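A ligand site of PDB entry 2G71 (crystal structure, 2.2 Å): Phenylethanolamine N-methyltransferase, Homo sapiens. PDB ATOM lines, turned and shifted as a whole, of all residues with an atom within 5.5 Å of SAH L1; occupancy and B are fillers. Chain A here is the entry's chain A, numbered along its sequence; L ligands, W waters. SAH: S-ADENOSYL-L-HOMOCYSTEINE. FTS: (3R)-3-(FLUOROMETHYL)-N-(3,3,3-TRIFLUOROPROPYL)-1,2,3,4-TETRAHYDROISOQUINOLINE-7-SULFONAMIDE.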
ATOM      1  N   VAL A  23     -18.778 -24.231 -37.633  1.00  0.00           N
ATOM      2  CA  VAL A  23     -18.727 -23.355 -36.464  1.00  0.00           C
ATOM      3  C   VAL A  23     -19.551 -22.117 -36.803  1.00  0.00           C
ATOM      4  O   VAL A  23     -20.465 -21.744 -36.056  1.00  0.00           O
ATOM      5  CB  VAL A  23     -17.262 -22.944 -36.138  1.00  0.00           C
ATOM      6  CG1 VAL A  23     -17.246 -21.739 -35.215  1.00  0.00           C
ATOM      7  CG2 VAL A  23     -16.522 -24.103 -35.495  1.00  0.00           C
ATOM      8  N   TYR A  27     -22.593 -20.256 -34.606  1.00  0.00           N
ATOM      9  CA  TYR A  27     -22.562 -18.883 -34.126  1.00  0.00           C
ATOM     10  C   TYR A  27     -23.757 -18.074 -34.583  1.00  0.00           C
ATOM     11  O   TYR A  27     -23.929 -16.916 -34.198  1.00  0.00           O
ATOM     12  CB  TYR A  27     -21.266 -18.177 -34.545  1.00  0.00           C
ATOM     13  CG  TYR A  27     -20.155 -18.388 -33.539  1.00  0.00           C
ATOM     14  CD1 TYR A  27     -19.137 -19.306 -33.794  1.00  0.00           C
ATOM     15  CD2 TYR A  27     -20.164 -17.733 -32.309  1.00  0.00           C
ATOM     16  CE1 TYR A  27     -18.159 -19.559 -32.835  1.00  0.00           C
ATOM     17  CE2 TYR A  27     -19.195 -17.987 -31.349  1.00  0.00           C
ATOM     18  CZ  TYR A  27     -18.198 -18.901 -31.613  1.00  0.00           C
ATOM     19  OH  TYR A  27     -17.265 -19.183 -30.651  1.00  0.00           O
ATOM     20  N   PHE A  30     -25.971 -17.585 -31.630  1.00  0.00           N
ATOM     21  CA  PHE A  30     -25.277 -16.871 -30.559  1.00  0.00           C
ATOM     22  C   PHE A  30     -26.083 -15.688 -30.034  1.00  0.00           C
ATOM     23  O   PHE A  30     -26.382 -14.760 -30.785  1.00  0.00           O
ATOM     24  CB  PHE A  30     -23.928 -16.380 -31.087  1.00  0.00           C
ATOM     25  CG  PHE A  30     -23.059 -15.736 -30.052  1.00  0.00           C
ATOM     26  CD1 PHE A  30     -22.095 -16.473 -29.370  1.00  0.00           C
ATOM     27  CD2 PHE A  30     -23.164 -14.367 -29.800  1.00  0.00           C
ATOM     28  CE1 PHE A  30     -21.252 -15.871 -28.439  1.00  0.00           C
ATOM     29  CE2 PHE A  30     -22.333 -13.753 -28.869  1.00  0.00           C
ATOM     30  CZ  PHE A  30     -21.367 -14.503 -28.188  1.00  0.00           C
ATOM     31  N   TYR A  35     -24.596 -14.363 -23.571  1.00  0.00           N
ATOM     32  CA  TYR A  35     -23.156 -14.478 -23.434  1.00  0.00           C
ATOM     33  C   TYR A  35     -22.663 -13.541 -22.319  1.00  0.00           C
ATOM     34  O   TYR A  35     -21.887 -13.944 -21.459  1.00  0.00           O
ATOM     35  CB  TYR A  35     -22.453 -14.113 -24.732  1.00  0.00           C
ATOM     36  CG  TYR A  35     -20.949 -14.157 -24.658  1.00  0.00           C
ATOM     37  CD1 TYR A  35     -20.262 -15.375 -24.717  1.00  0.00           C
ATOM     38  CD2 TYR A  35     -20.204 -12.980 -24.515  1.00  0.00           C
ATOM     39  CE1 TYR A  35     -18.879 -15.417 -24.657  1.00  0.00           C
ATOM     40  CE2 TYR A  35     -18.811 -13.020 -24.454  1.00  0.00           C
ATOM     41  CZ  TYR A  35     -18.154 -14.236 -24.522  1.00  0.00           C
ATOM     42  OH  TYR A  35     -16.778 -14.277 -24.504  1.00  0.00           O
ATOM     43  N   TYR A  40     -20.049 -12.098 -17.875  1.00  0.00           N
ATOM     44  CA  TYR A  40     -19.730 -10.789 -17.317  1.00  0.00           C
ATOM     45  C   TYR A  40     -20.604 -10.271 -16.175  1.00  0.00           C
ATOM     46  O   TYR A  40     -20.390  -9.163 -15.678  1.00  0.00           O
ATOM     47  CB  TYR A  40     -19.617  -9.780 -18.485  1.00  0.00           C
ATOM     48  CG  TYR A  40     -18.510 -10.198 -19.422  1.00  0.00           C
ATOM     49  CD1 TYR A  40     -18.725 -11.146 -20.413  1.00  0.00           C
ATOM     50  CD2 TYR A  40     -17.212  -9.781 -19.191  1.00  0.00           C
ATOM     51  CE1 TYR A  40     -17.644 -11.679 -21.146  1.00  0.00           C
ATOM     52  CE2 TYR A  40     -16.142 -10.317 -19.910  1.00  0.00           C
ATOM     53  CZ  TYR A  40     -16.360 -11.259 -20.866  1.00  0.00           C
ATOM     54  OH  TYR A  40     -15.263 -11.817 -21.478  1.00  0.00           O
ATOM     55  N   LYS A  57      -7.823 -10.748 -15.067  1.00  0.00           N
ATOM     56  CA  LYS A  57      -7.703 -10.323 -16.447  1.00  0.00           C
ATOM     57  C   LYS A  57      -7.374  -8.843 -16.566  1.00  0.00           C
ATOM     58  O   LYS A  57      -6.478  -8.465 -17.320  1.00  0.00           O
ATOM     59  CB  LYS A  57      -8.980 -10.623 -17.237  1.00  0.00           C
ATOM     60  CG  LYS A  57      -9.180 -12.106 -17.508  1.00  0.00           C
ATOM     61  CD  LYS A  57     -10.145 -12.357 -18.667  1.00  0.00           C
ATOM     62  CE  LYS A  57     -11.504 -11.814 -18.341  1.00  0.00           C
ATOM     63  NZ  LYS A  57     -12.583 -12.065 -19.322  1.00  0.00           N
ATOM     64  N   ASP A  77      -9.028  -4.727 -32.234  1.00  0.00           N
ATOM     65  CA  ASP A  77      -9.500  -5.739 -31.300  1.00  0.00           C
ATOM     66  C   ASP A  77     -10.193  -6.809 -32.137  1.00  0.00           C
ATOM     67  O   ASP A  77     -11.216  -6.552 -32.758  1.00  0.00           O
ATOM     68  CB  ASP A  77     -10.480  -5.140 -30.281  1.00  0.00           C
ATOM     69  CG  ASP A  77     -10.965  -6.166 -29.257  1.00  0.00           C
ATOM     70  OD1 ASP A  77     -10.142  -6.993 -28.823  1.00  0.00           O
ATOM     71  OD2 ASP A  77     -12.161  -6.151 -28.889  1.00  0.00           O
ATOM     72  N   ILE A  78      -9.604  -8.011 -32.137  1.00  0.00           N
ATOM     73  CA  ILE A  78     -10.097  -9.159 -32.902  1.00  0.00           C
ATOM     74  C   ILE A  78     -11.182  -9.932 -32.176  1.00  0.00           C
ATOM     75  O   ILE A  78     -10.972 -10.398 -31.055  1.00  0.00           O
ATOM     76  CB  ILE A  78      -8.962 -10.156 -33.197  1.00  0.00           C
ATOM     77  CG1 ILE A  78      -7.707  -9.417 -33.680  1.00  0.00           C
ATOM     78  CG2 ILE A  78      -9.437 -11.181 -34.216  1.00  0.00           C
ATOM     79  CD1 ILE A  78      -7.861  -8.695 -35.017  1.00  0.00           C
ATOM     80  N   GLY A  79     -12.339 -10.097 -32.816  1.00  0.00           N
ATOM     81  CA  GLY A  79     -13.439 -10.838 -32.217  1.00  0.00           C
ATOM     82  C   GLY A  79     -13.894 -10.224 -30.909  1.00  0.00           C
ATOM     83  O   GLY A  79     -14.066 -10.911 -29.917  1.00  0.00           O
ATOM     84  N   SER A  80     -14.112  -8.909 -30.944  1.00  0.00           N
ATOM     85  CA  SER A  80     -14.539  -8.155 -29.769  1.00  0.00           C
ATOM     86  C   SER A  80     -15.827  -8.683 -29.154  1.00  0.00           C
ATOM     87  O   SER A  80     -16.046  -8.542 -27.946  1.00  0.00           O
ATOM     88  CB  SER A  80     -14.748  -6.685 -30.156  1.00  0.00           C
ATOM     89  OG  SER A  80     -13.626  -6.166 -30.838  1.00  0.00           O
ATOM     90  N   GLY A  81     -16.679  -9.285 -29.965  1.00  0.00           N
ATOM     91  CA  GLY A  81     -17.950  -9.756 -29.439  1.00  0.00           C
ATOM     92  C   GLY A  81     -18.708  -8.558 -28.903  1.00  0.00           C
ATOM     93  O   GLY A  81     -18.564  -7.454 -29.432  1.00  0.00           O
ATOM     94  N   PRO A  82     -19.516  -8.729 -27.840  1.00  0.00           N
ATOM     95  CA  PRO A  82     -20.273  -7.611 -27.274  1.00  0.00           C
ATOM     96  C   PRO A  82     -19.603  -7.009 -26.055  1.00  0.00           C
ATOM     97  O   PRO A  82     -20.275  -6.415 -25.209  1.00  0.00           O
ATOM     98  CB  PRO A  82     -21.597  -8.255 -26.902  1.00  0.00           C
ATOM     99  CG  PRO A  82     -21.137  -9.583 -26.371  1.00  0.00           C
ATOM    100  CD  PRO A  82     -20.065 -10.012 -27.361  1.00  0.00           C
ATOM    101  N   THR A  83     -18.288  -7.150 -25.948  1.00  0.00           N
ATOM    102  CA  THR A  83     -17.590  -6.635 -24.768  1.00  0.00           C
ATOM    103  C   THR A  83     -16.540  -5.579 -25.075  1.00  0.00           C
ATOM    104  O   THR A  83     -16.005  -5.523 -26.175  1.00  0.00           O
ATOM    105  CB  THR A  83     -16.920  -7.804 -23.981  1.00  0.00           C
ATOM    106  OG1 THR A  83     -15.712  -8.213 -24.634  1.00  0.00           O
ATOM    107  CG2 THR A  83     -17.883  -8.993 -23.890  1.00  0.00           C
ATOM    108  N   TYR A  85     -14.345  -4.443 -22.058  1.00  0.00           N
ATOM    109  CA  TYR A  85     -13.385  -4.462 -20.943  1.00  0.00           C
ATOM    110  C   TYR A  85     -11.955  -4.685 -21.416  1.00  0.00           C
ATOM    111  O   TYR A  85     -11.012  -4.203 -20.777  1.00  0.00           O
ATOM    112  CB  TYR A  85     -13.734  -5.573 -19.937  1.00  0.00           C
ATOM    113  CG  TYR A  85     -13.364  -6.966 -20.437  1.00  0.00           C
ATOM    114  CD1 TYR A  85     -12.057  -7.455 -20.281  1.00  0.00           C
ATOM    115  CD2 TYR A  85     -14.277  -7.725 -21.162  1.00  0.00           C
ATOM    116  CE1 TYR A  85     -11.690  -8.672 -20.856  1.00  0.00           C
ATOM    117  CE2 TYR A  85     -13.910  -8.942 -21.737  1.00  0.00           C
ATOM    118  CZ  TYR A  85     -12.617  -9.405 -21.594  1.00  0.00           C
ATOM    119  OH  TYR A  85     -12.264 -10.587 -22.189  1.00  0.00           O
ATOM    120  N   GLN A  86     -11.801  -5.423 -22.515  1.00  0.00           N
ATOM    121  CA  GLN A  86     -10.476  -5.733 -23.028  1.00  0.00           C
ATOM    122  C   GLN A  86      -9.744  -4.537 -23.608  1.00  0.00           C
ATOM    123  O   GLN A  86      -8.577  -4.629 -23.969  1.00  0.00           O
ATOM    124  CB  GLN A  86     -10.558  -6.850 -24.085  1.00  0.00           C
ATOM    125  CG  GLN A  86     -11.270  -6.464 -25.390  1.00  0.00           C
ATOM    126  CD  GLN A  86     -12.762  -6.732 -25.362  1.00  0.00           C
ATOM    127  OE1 GLN A  86     -13.390  -6.758 -24.308  1.00  0.00           O
ATOM    128  NE2 GLN A  86     -13.338  -6.926 -26.543  1.00  0.00           N
ATOM    129  N   ASP A 101     -15.912  -8.056 -35.182  1.00  0.00           N
ATOM    130  CA  ASP A 101     -16.628  -9.285 -34.894  1.00  0.00           C
ATOM    131  C   ASP A 101     -17.355  -9.862 -36.094  1.00  0.00           C
ATOM    132  O   ASP A 101     -17.784  -9.142 -36.985  1.00  0.00           O
ATOM    133  CB  ASP A 101     -17.616  -9.130 -33.753  1.00  0.00           C
ATOM    134  CG  ASP A 101     -17.879 -10.449 -33.059  1.00  0.00           C
ATOM    135  OD1 ASP A 101     -16.932 -10.943 -32.406  1.00  0.00           O
ATOM    136  OD2 ASP A 101     -19.003 -10.986 -33.173  1.00  0.00           O
ATOM    137  N   PHE A 102     -17.478 -11.188 -36.080  1.00  0.00           N
ATOM    138  CA  PHE A 102     -18.115 -11.943 -37.143  1.00  0.00           C
ATOM    139  C   PHE A 102     -19.626 -11.768 -37.132  1.00  0.00           C
ATOM    140  O   PHE A 102     -20.278 -11.867 -38.170  1.00  0.00           O
ATOM    141  CB  PHE A 102     -17.770 -13.417 -36.954  1.00  0.00           C
ATOM    142  CG  PHE A 102     -18.341 -14.335 -37.993  1.00  0.00           C
ATOM    143  CD1 PHE A 102     -17.760 -14.436 -39.242  1.00  0.00           C
ATOM    144  CD2 PHE A 102     -19.455 -15.113 -37.702  1.00  0.00           C
ATOM    145  CE1 PHE A 102     -18.283 -15.314 -40.198  1.00  0.00           C
ATOM    146  CE2 PHE A 102     -19.989 -15.993 -38.646  1.00  0.00           C
ATOM    147  CZ  PHE A 102     -19.399 -16.086 -39.900  1.00  0.00           C
ATOM    148  N   LEU A 103     -20.195 -11.518 -35.959  1.00  0.00           N
ATOM    149  CA  LEU A 103     -21.637 -11.372 -35.853  1.00  0.00           C
ATOM    150  C   LEU A 103     -22.169  -9.952 -35.858  1.00  0.00           C
ATOM    151  O   LEU A 103     -21.680  -9.076 -35.138  1.00  0.00           O
ATOM    152  CB  LEU A 103     -22.138 -12.090 -34.592  1.00  0.00           C
ATOM    153  CG  LEU A 103     -22.016 -13.605 -34.603  1.00  0.00           C
ATOM    154  CD1 LEU A 103     -22.560 -14.196 -33.302  1.00  0.00           C
ATOM    155  CD2 LEU A 103     -22.797 -14.154 -35.812  1.00  0.00           C
ATOM    156  N   ASN A 106     -23.451  -8.807 -32.504  1.00  0.00           N
ATOM    157  CA  ASN A 106     -22.448  -8.308 -31.584  1.00  0.00           C
ATOM    158  C   ASN A 106     -22.022  -6.894 -31.921  1.00  0.00           C
ATOM    159  O   ASN A 106     -21.863  -6.065 -31.025  1.00  0.00           O
ATOM    160  CB  ASN A 106     -21.211  -9.205 -31.541  1.00  0.00           C
ATOM    161  CG  ASN A 106     -21.428 -10.437 -30.697  1.00  0.00           C
ATOM    162  OD1 ASN A 106     -22.068 -10.378 -29.654  1.00  0.00           O
ATOM    163  ND2 ASN A 106     -20.890 -11.568 -31.136  1.00  0.00           N
ATOM    164  N   ILE A 157     -15.413  -9.250 -39.417  1.00  0.00           N
ATOM    165  CA  ILE A 157     -14.135  -9.929 -39.585  1.00  0.00           C
ATOM    166  C   ILE A 157     -14.354 -11.432 -39.532  1.00  0.00           C
ATOM    167  O   ILE A 157     -15.371 -11.903 -39.018  1.00  0.00           O
ATOM    168  CB  ILE A 157     -13.147  -9.485 -38.470  1.00  0.00           C
ATOM    169  CG1 ILE A 157     -11.804 -10.197 -38.623  1.00  0.00           C
ATOM    170  CG2 ILE A 157     -13.744  -9.779 -37.105  1.00  0.00           C
ATOM    171  CD1 ILE A 157     -10.738  -9.660 -37.682  1.00  0.00           C
ATOM    172  N   ASP A 158     -13.403 -12.181 -40.086  1.00  0.00           N
ATOM    173  CA  ASP A 158     -13.453 -13.637 -40.104  1.00  0.00           C
ATOM    174  C   ASP A 158     -12.019 -14.115 -40.053  1.00  0.00           C
ATOM    175  O   ASP A 158     -11.334 -14.139 -41.077  1.00  0.00           O
ATOM    176  CB  ASP A 158     -14.102 -14.146 -41.401  1.00  0.00           C
ATOM    177  CG  ASP A 158     -14.201 -15.659 -41.447  1.00  0.00           C
ATOM    178  OD1 ASP A 158     -13.454 -16.341 -40.697  1.00  0.00           O
ATOM    179  OD2 ASP A 158     -15.017 -16.177 -42.244  1.00  0.00           O
ATOM    180  N   VAL A 159     -11.563 -14.500 -38.870  1.00  0.00           N
ATOM    181  CA  VAL A 159     -10.182 -14.948 -38.721  1.00  0.00           C
ATOM    182  C   VAL A 159      -9.855 -16.149 -39.616  1.00  0.00           C
ATOM    183  O   VAL A 159      -8.682 -16.470 -39.827  1.00  0.00           O
ATOM    184  CB  VAL A 159      -9.874 -15.293 -37.253  1.00  0.00           C
ATOM    185  CG1 VAL A 159      -9.944 -14.026 -36.402  1.00  0.00           C
ATOM    186  CG2 VAL A 159     -10.859 -16.333 -36.743  1.00  0.00           C
ATOM    187  N   HIS A 160     -10.870 -16.813 -40.136  1.00  0.00           N
ATOM    188  CA  HIS A 160     -10.633 -17.974 -40.992  1.00  0.00           C
ATOM    189  C   HIS A 160     -10.188 -17.601 -42.405  1.00  0.00           C
ATOM    190  O   HIS A 160      -9.743 -18.467 -43.153  1.00  0.00           O
ATOM    191  CB  HIS A 160     -11.867 -18.869 -41.042  1.00  0.00           C
ATOM    192  CG  HIS A 160     -12.203 -19.498 -39.730  1.00  0.00           C
ATOM    193  ND1 HIS A 160     -11.245 -20.119 -38.949  1.00  0.00           N
ATOM    194  CD2 HIS A 160     -13.370 -19.608 -39.055  1.00  0.00           C
ATOM    195  CE1 HIS A 160     -11.816 -20.582 -37.847  1.00  0.00           C
ATOM    196  NE2 HIS A 160     -13.108 -20.290 -37.894  1.00  0.00           N
ATOM    197  N   ALA A 181      -9.436 -11.510 -27.253  1.00  0.00           N
ATOM    198  CA  ALA A 181      -9.815 -12.254 -26.078  1.00  0.00           C
ATOM    199  C   ALA A 181     -10.910 -13.289 -26.340  1.00  0.00           C
ATOM    200  O   ALA A 181     -11.999 -12.942 -26.797  1.00  0.00           O
ATOM    201  CB  ALA A 181     -10.270 -11.293 -24.970  1.00  0.00           C
ATOM    202  N   PHE A 182     -10.596 -14.550 -26.048  1.00  0.00           N
ATOM    203  CA  PHE A 182     -11.534 -15.649 -26.220  1.00  0.00           C
ATOM    204  C   PHE A 182     -12.110 -15.819 -27.613  1.00  0.00           C
ATOM    205  O   PHE A 182     -13.262 -16.222 -27.770  1.00  0.00           O
ATOM    206  CB  PHE A 182     -12.683 -15.507 -25.223  1.00  0.00           C
ATOM    207  CG  PHE A 182     -12.228 -15.416 -23.800  1.00  0.00           C
ATOM    208  CD1 PHE A 182     -12.156 -14.188 -23.155  1.00  0.00           C
ATOM    209  CD2 PHE A 182     -11.888 -16.578 -23.103  1.00  0.00           C
ATOM    210  CE1 PHE A 182     -11.756 -14.102 -21.820  1.00  0.00           C
ATOM    211  CE2 PHE A 182     -11.485 -16.506 -21.768  1.00  0.00           C
ATOM    212  CZ  PHE A 182     -11.415 -15.264 -21.123  1.00  0.00           C
ATOM    213  N   CYS A 183     -11.326 -15.510 -28.640  1.00  0.00           N
ATOM    214  CA  CYS A 183     -11.821 -15.633 -29.990  1.00  0.00           C
ATOM    215  C   CYS A 183     -11.307 -16.876 -30.714  1.00  0.00           C
ATOM    216  O   CYS A 183     -12.071 -17.805 -30.999  1.00  0.00           O
ATOM    217  CB  CYS A 183     -11.454 -14.399 -30.803  1.00  0.00           C
ATOM    218  SG  CYS A 183     -12.045 -14.469 -32.504  1.00  0.00           S
ATOM    219  N   ALA A 186     -12.239 -20.243 -29.536  1.00  0.00           N
ATOM    220  CA  ALA A 186     -13.703 -20.329 -29.608  1.00  0.00           C
ATOM    221  C   ALA A 186     -14.258 -20.494 -31.014  1.00  0.00           C
ATOM    222  O   ALA A 186     -15.436 -20.801 -31.182  1.00  0.00           O
ATOM    223  CB  ALA A 186     -14.310 -19.096 -28.990  1.00  0.00           C
ATOM    224  N   VAL A 187     -13.429 -20.280 -32.030  1.00  0.00           N
ATOM    225  CA  VAL A 187     -13.904 -20.390 -33.414  1.00  0.00           C
ATOM    226  C   VAL A 187     -13.160 -21.440 -34.233  1.00  0.00           C
ATOM    227  O   VAL A 187     -13.443 -21.629 -35.411  1.00  0.00           O
ATOM    228  CB  VAL A 187     -13.789 -19.023 -34.128  1.00  0.00           C
ATOM    229  CG1 VAL A 187     -14.362 -17.934 -33.225  1.00  0.00           C
ATOM    230  CG2 VAL A 187     -12.342 -18.711 -34.476  1.00  0.00           C
ATOM    231  N   TYR A 222     -19.052 -24.035 -24.751  1.00  0.00           N
ATOM    232  CA  TYR A 222     -19.578 -22.949 -23.931  1.00  0.00           C
ATOM    233  C   TYR A 222     -20.933 -22.605 -24.511  1.00  0.00           C
ATOM    234  O   TYR A 222     -21.174 -22.794 -25.708  1.00  0.00           O
ATOM    235  CB  TYR A 222     -18.649 -21.729 -23.909  1.00  0.00           C
ATOM    236  CG  TYR A 222     -18.677 -20.834 -25.128  1.00  0.00           C
ATOM    237  CD1 TYR A 222     -19.450 -19.676 -25.142  1.00  0.00           C
ATOM    238  CD2 TYR A 222     -17.865 -21.106 -26.231  1.00  0.00           C
ATOM    239  CE1 TYR A 222     -19.404 -18.798 -26.223  1.00  0.00           C
ATOM    240  CE2 TYR A 222     -17.818 -20.234 -27.319  1.00  0.00           C
ATOM    241  CZ  TYR A 222     -18.582 -19.084 -27.297  1.00  0.00           C
ATOM    242  OH  TYR A 222     -18.522 -18.183 -28.340  1.00  0.00           O
HETATM  243  N   SAH L   1     -13.747 -11.075 -27.133  1.00  0.00           N
HETATM  244  CA  SAH L   1     -14.985 -11.165 -26.369  1.00  0.00           C
HETATM  245  CB  SAH L   1     -15.933 -12.177 -27.026  1.00  0.00           C
HETATM  246  CG  SAH L   1     -15.379 -13.584 -27.217  1.00  0.00           C
HETATM  247  SD  SAH L   1     -16.673 -14.732 -27.718  1.00  0.00           S
HETATM  248  C   SAH L   1     -14.708 -11.507 -24.896  1.00  0.00           C
HETATM  249  O   SAH L   1     -13.565 -11.292 -24.452  1.00  0.00           O
HETATM  250  OXT SAH L   1     -15.637 -11.967 -24.199  1.00  0.00           O
HETATM  251  C5' SAH L   1     -16.081 -15.236 -29.352  1.00  0.00           C
HETATM  252  C4' SAH L   1     -16.416 -14.206 -30.418  1.00  0.00           C
HETATM  253  O4' SAH L   1     -15.831 -14.563 -31.709  1.00  0.00           O
HETATM  254  C3' SAH L   1     -17.900 -13.956 -30.670  1.00  0.00           C
HETATM  255  O3' SAH L   1     -18.191 -12.567 -30.570  1.00  0.00           O
HETATM  256  C2' SAH L   1     -18.127 -14.527 -32.066  1.00  0.00           C
HETATM  257  O2' SAH L   1     -19.162 -13.893 -32.794  1.00  0.00           O
HETATM  258  C1' SAH L   1     -16.773 -14.266 -32.714  1.00  0.00           C
HETATM  259  N9  SAH L   1     -16.480 -15.063 -33.907  1.00  0.00           N
HETATM  260  C8  SAH L   1     -17.121 -16.243 -34.378  1.00  0.00           C
HETATM  261  N7  SAH L   1     -16.623 -16.701 -35.503  1.00  0.00           N
HETATM  262  C5  SAH L   1     -15.611 -15.796 -35.793  1.00  0.00           C
HETATM  263  C6  SAH L   1     -14.725 -15.776 -36.895  1.00  0.00           C
HETATM  264  N6  SAH L   1     -14.734 -16.683 -37.878  1.00  0.00           N
HETATM  265  N1  SAH L   1     -13.819 -14.757 -36.943  1.00  0.00           N
HETATM  266  C2  SAH L   1     -13.814 -13.837 -35.944  1.00  0.00           C
HETATM  267  N3  SAH L   1     -14.612 -13.771 -34.846  1.00  0.00           N
HETATM  268  C4  SAH L   1     -15.492 -14.805 -34.833  1.00  0.00           C
HETATM  269  C7  FTS L   2     -14.480 -17.319 -19.762  1.00  0.00           C
HETATM  270  C8  FTS L   2     -14.931 -17.762 -21.008  1.00  0.00           C
HETATM  271  C1  FTS L   2     -14.921 -19.265 -21.324  1.00  0.00           C
HETATM  272  N1  FTS L   2     -15.697 -19.534 -22.536  1.00  0.00           N
HETATM  273  C2  FTS L   2     -15.247 -18.688 -23.651  1.00  0.00           C
HETATM  274  C10 FTS L   2     -15.733 -19.247 -24.991  1.00  0.00           C
HETATM  275  F4  FTS L   2     -15.217 -18.538 -26.010  1.00  0.00           F
HETATM  276  C3  FTS L   2     -15.786 -17.291 -23.353  1.00  0.00           C
HETATM  277  C9  FTS L   2     -15.326 -16.840 -21.964  1.00  0.00           C
HETATM  278  C4  FTS L   2     -15.292 -15.479 -21.661  1.00  0.00           C
HETATM  279  C5  FTS L   2     -14.842 -15.028 -20.422  1.00  0.00           C
HETATM  280  C6  FTS L   2     -14.446 -15.950 -19.466  1.00  0.00           C
HETATM  281  S1  FTS L   2     -13.889 -15.435 -17.883  1.00  0.00           S
HETATM  282  O1  FTS L   2     -12.481 -15.752 -17.831  1.00  0.00           O
HETATM  283  O2  FTS L   2     -14.751 -16.055 -16.908  1.00  0.00           O
HETATM  284  N2  FTS L   2     -13.996 -13.833 -17.703  1.00  0.00           N
HETATM  285  C11 FTS L   2     -15.275 -13.275 -17.251  1.00  0.00           C
HETATM  286  C12 FTS L   2     -15.223 -12.529 -15.926  1.00  0.00           C
HETATM  287  C13 FTS L   2     -14.772 -11.107 -15.914  1.00  0.00           C
HETATM  288  F1  FTS L   2     -14.937 -10.467 -14.743  1.00  0.00           F
HETATM  289  F2  FTS L   2     -15.448 -10.322 -16.767  1.00  0.00           F
HETATM  290  F3  FTS L   2     -13.490 -10.908 -16.264  1.00  0.00           F
HETATM  291  O   HOH W   1     -11.478  -9.470 -28.277  1.00  0.00           O
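O of Gly 79 sits at hydrogen-bond distance from N of SAH L1 (2.8 Å). The backbone carbonyl oxygen of Ala 181 sits at hydrogen-bond distance from a nitrogen (N) of SAH L1. OXT of SAH L1 is in hydrogen-bond range of OH of Tyr 35, 2.6 Å away. O3' of SAH L1 sits at hydrogen-bond distance from OD1 of Asp 101 (2.8 Å). N of Val 159 sits at hydrogen-bond distance from N1 of SAH L1, 3.0 Å away. The side-chain sulfur (SG) of Cys 183 is in hydrogen-bond range of a nitrogen (N3) of SAH L1, 3.5 Å away. An oxygen (O3') of SAH L1 is in hydrogen-bond range of the side-chain amide nitrogen (ND2) of Asn 106 (2.9 Å). The side-chain hydroxyl (OH) of Tyr 85 sits at hydrogen-bond distance from an oxygen (O) of SAH L1 (2.7 Å). OH of Tyr 40 is in hydrogen-bond range of OXT of SAH L1 (2.8 Å). A nitrogen (N6) of SAH L1 is in hydrogen-bond range of the side-chain carboxylate (OD1) of Asp 158, at 3.1 Å.
The backbone carbonyl oxygen (O) of Ser 80 sits at hydrogen-bond distance from the side-chain amide nitrogen (NE2) of Gln 86 (3.5 Å). The side-chain amino group of Lys 57 lies within hydrogen-bond range of the side-chain hydroxyl of Tyr 40 (3.4 Å). OH of Tyr 27 sits at hydrogen-bond distance from O of Ala 186 (2.5 Å). OG of Ser 80 is in hydrogen-bond range of OD2 of Asp 77 (2.4 Å). The side-chain carboxylate (OD1) of Asp 101 lies within hydrogen-bond range of the backbone NH (N) of Gly 81 (3.0 Å). The side-chain carboxylate of Asp 158 sits at hydrogen-bond distance from the backbone NH of His 160. The backbone NH (N) of Ile 157 is in hydrogen-bond range of the backbone carbonyl oxygen (O) of Asp 101, at 3.4 Å. OH of Tyr 85 lies close to OH of Tyr 40, 3.3 Å away.
O of Phe 182 lies close to SD of SAH L1, at 3.7 Å. CE2 of Tyr 27 touches C2' of SAH L1 (3.7 Å). Ser 80 touches SAH L1. CA of Gly 81 touches O3' of SAH L1 (3.0 Å). Thr 83 touches SAH L1. CB of Phe 102 touches C4 of SAH L1 (3.4 Å). CG of Leu 103 touches O2' of SAH L1 (3.4 Å). Ile 157 touches SAH L1. CD2 of His 160 touches N6 of SAH L1, at 3.4 Å. CG1 of Val 187 touches C8 of SAH L1, at 3.4 Å. Tyr 222 touches SAH L1. Hydrophobic or aromatic side chains within 4 Å of SAH L1: Tyr 27, Tyr 35, Tyr 40, Tyr 85, Phe 102, Leu 103, Val 159, His 160, Ala 181, Phe 182 and Val 187. Of the 29 residues printed, 21 come within 4 Å of SAH L1.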
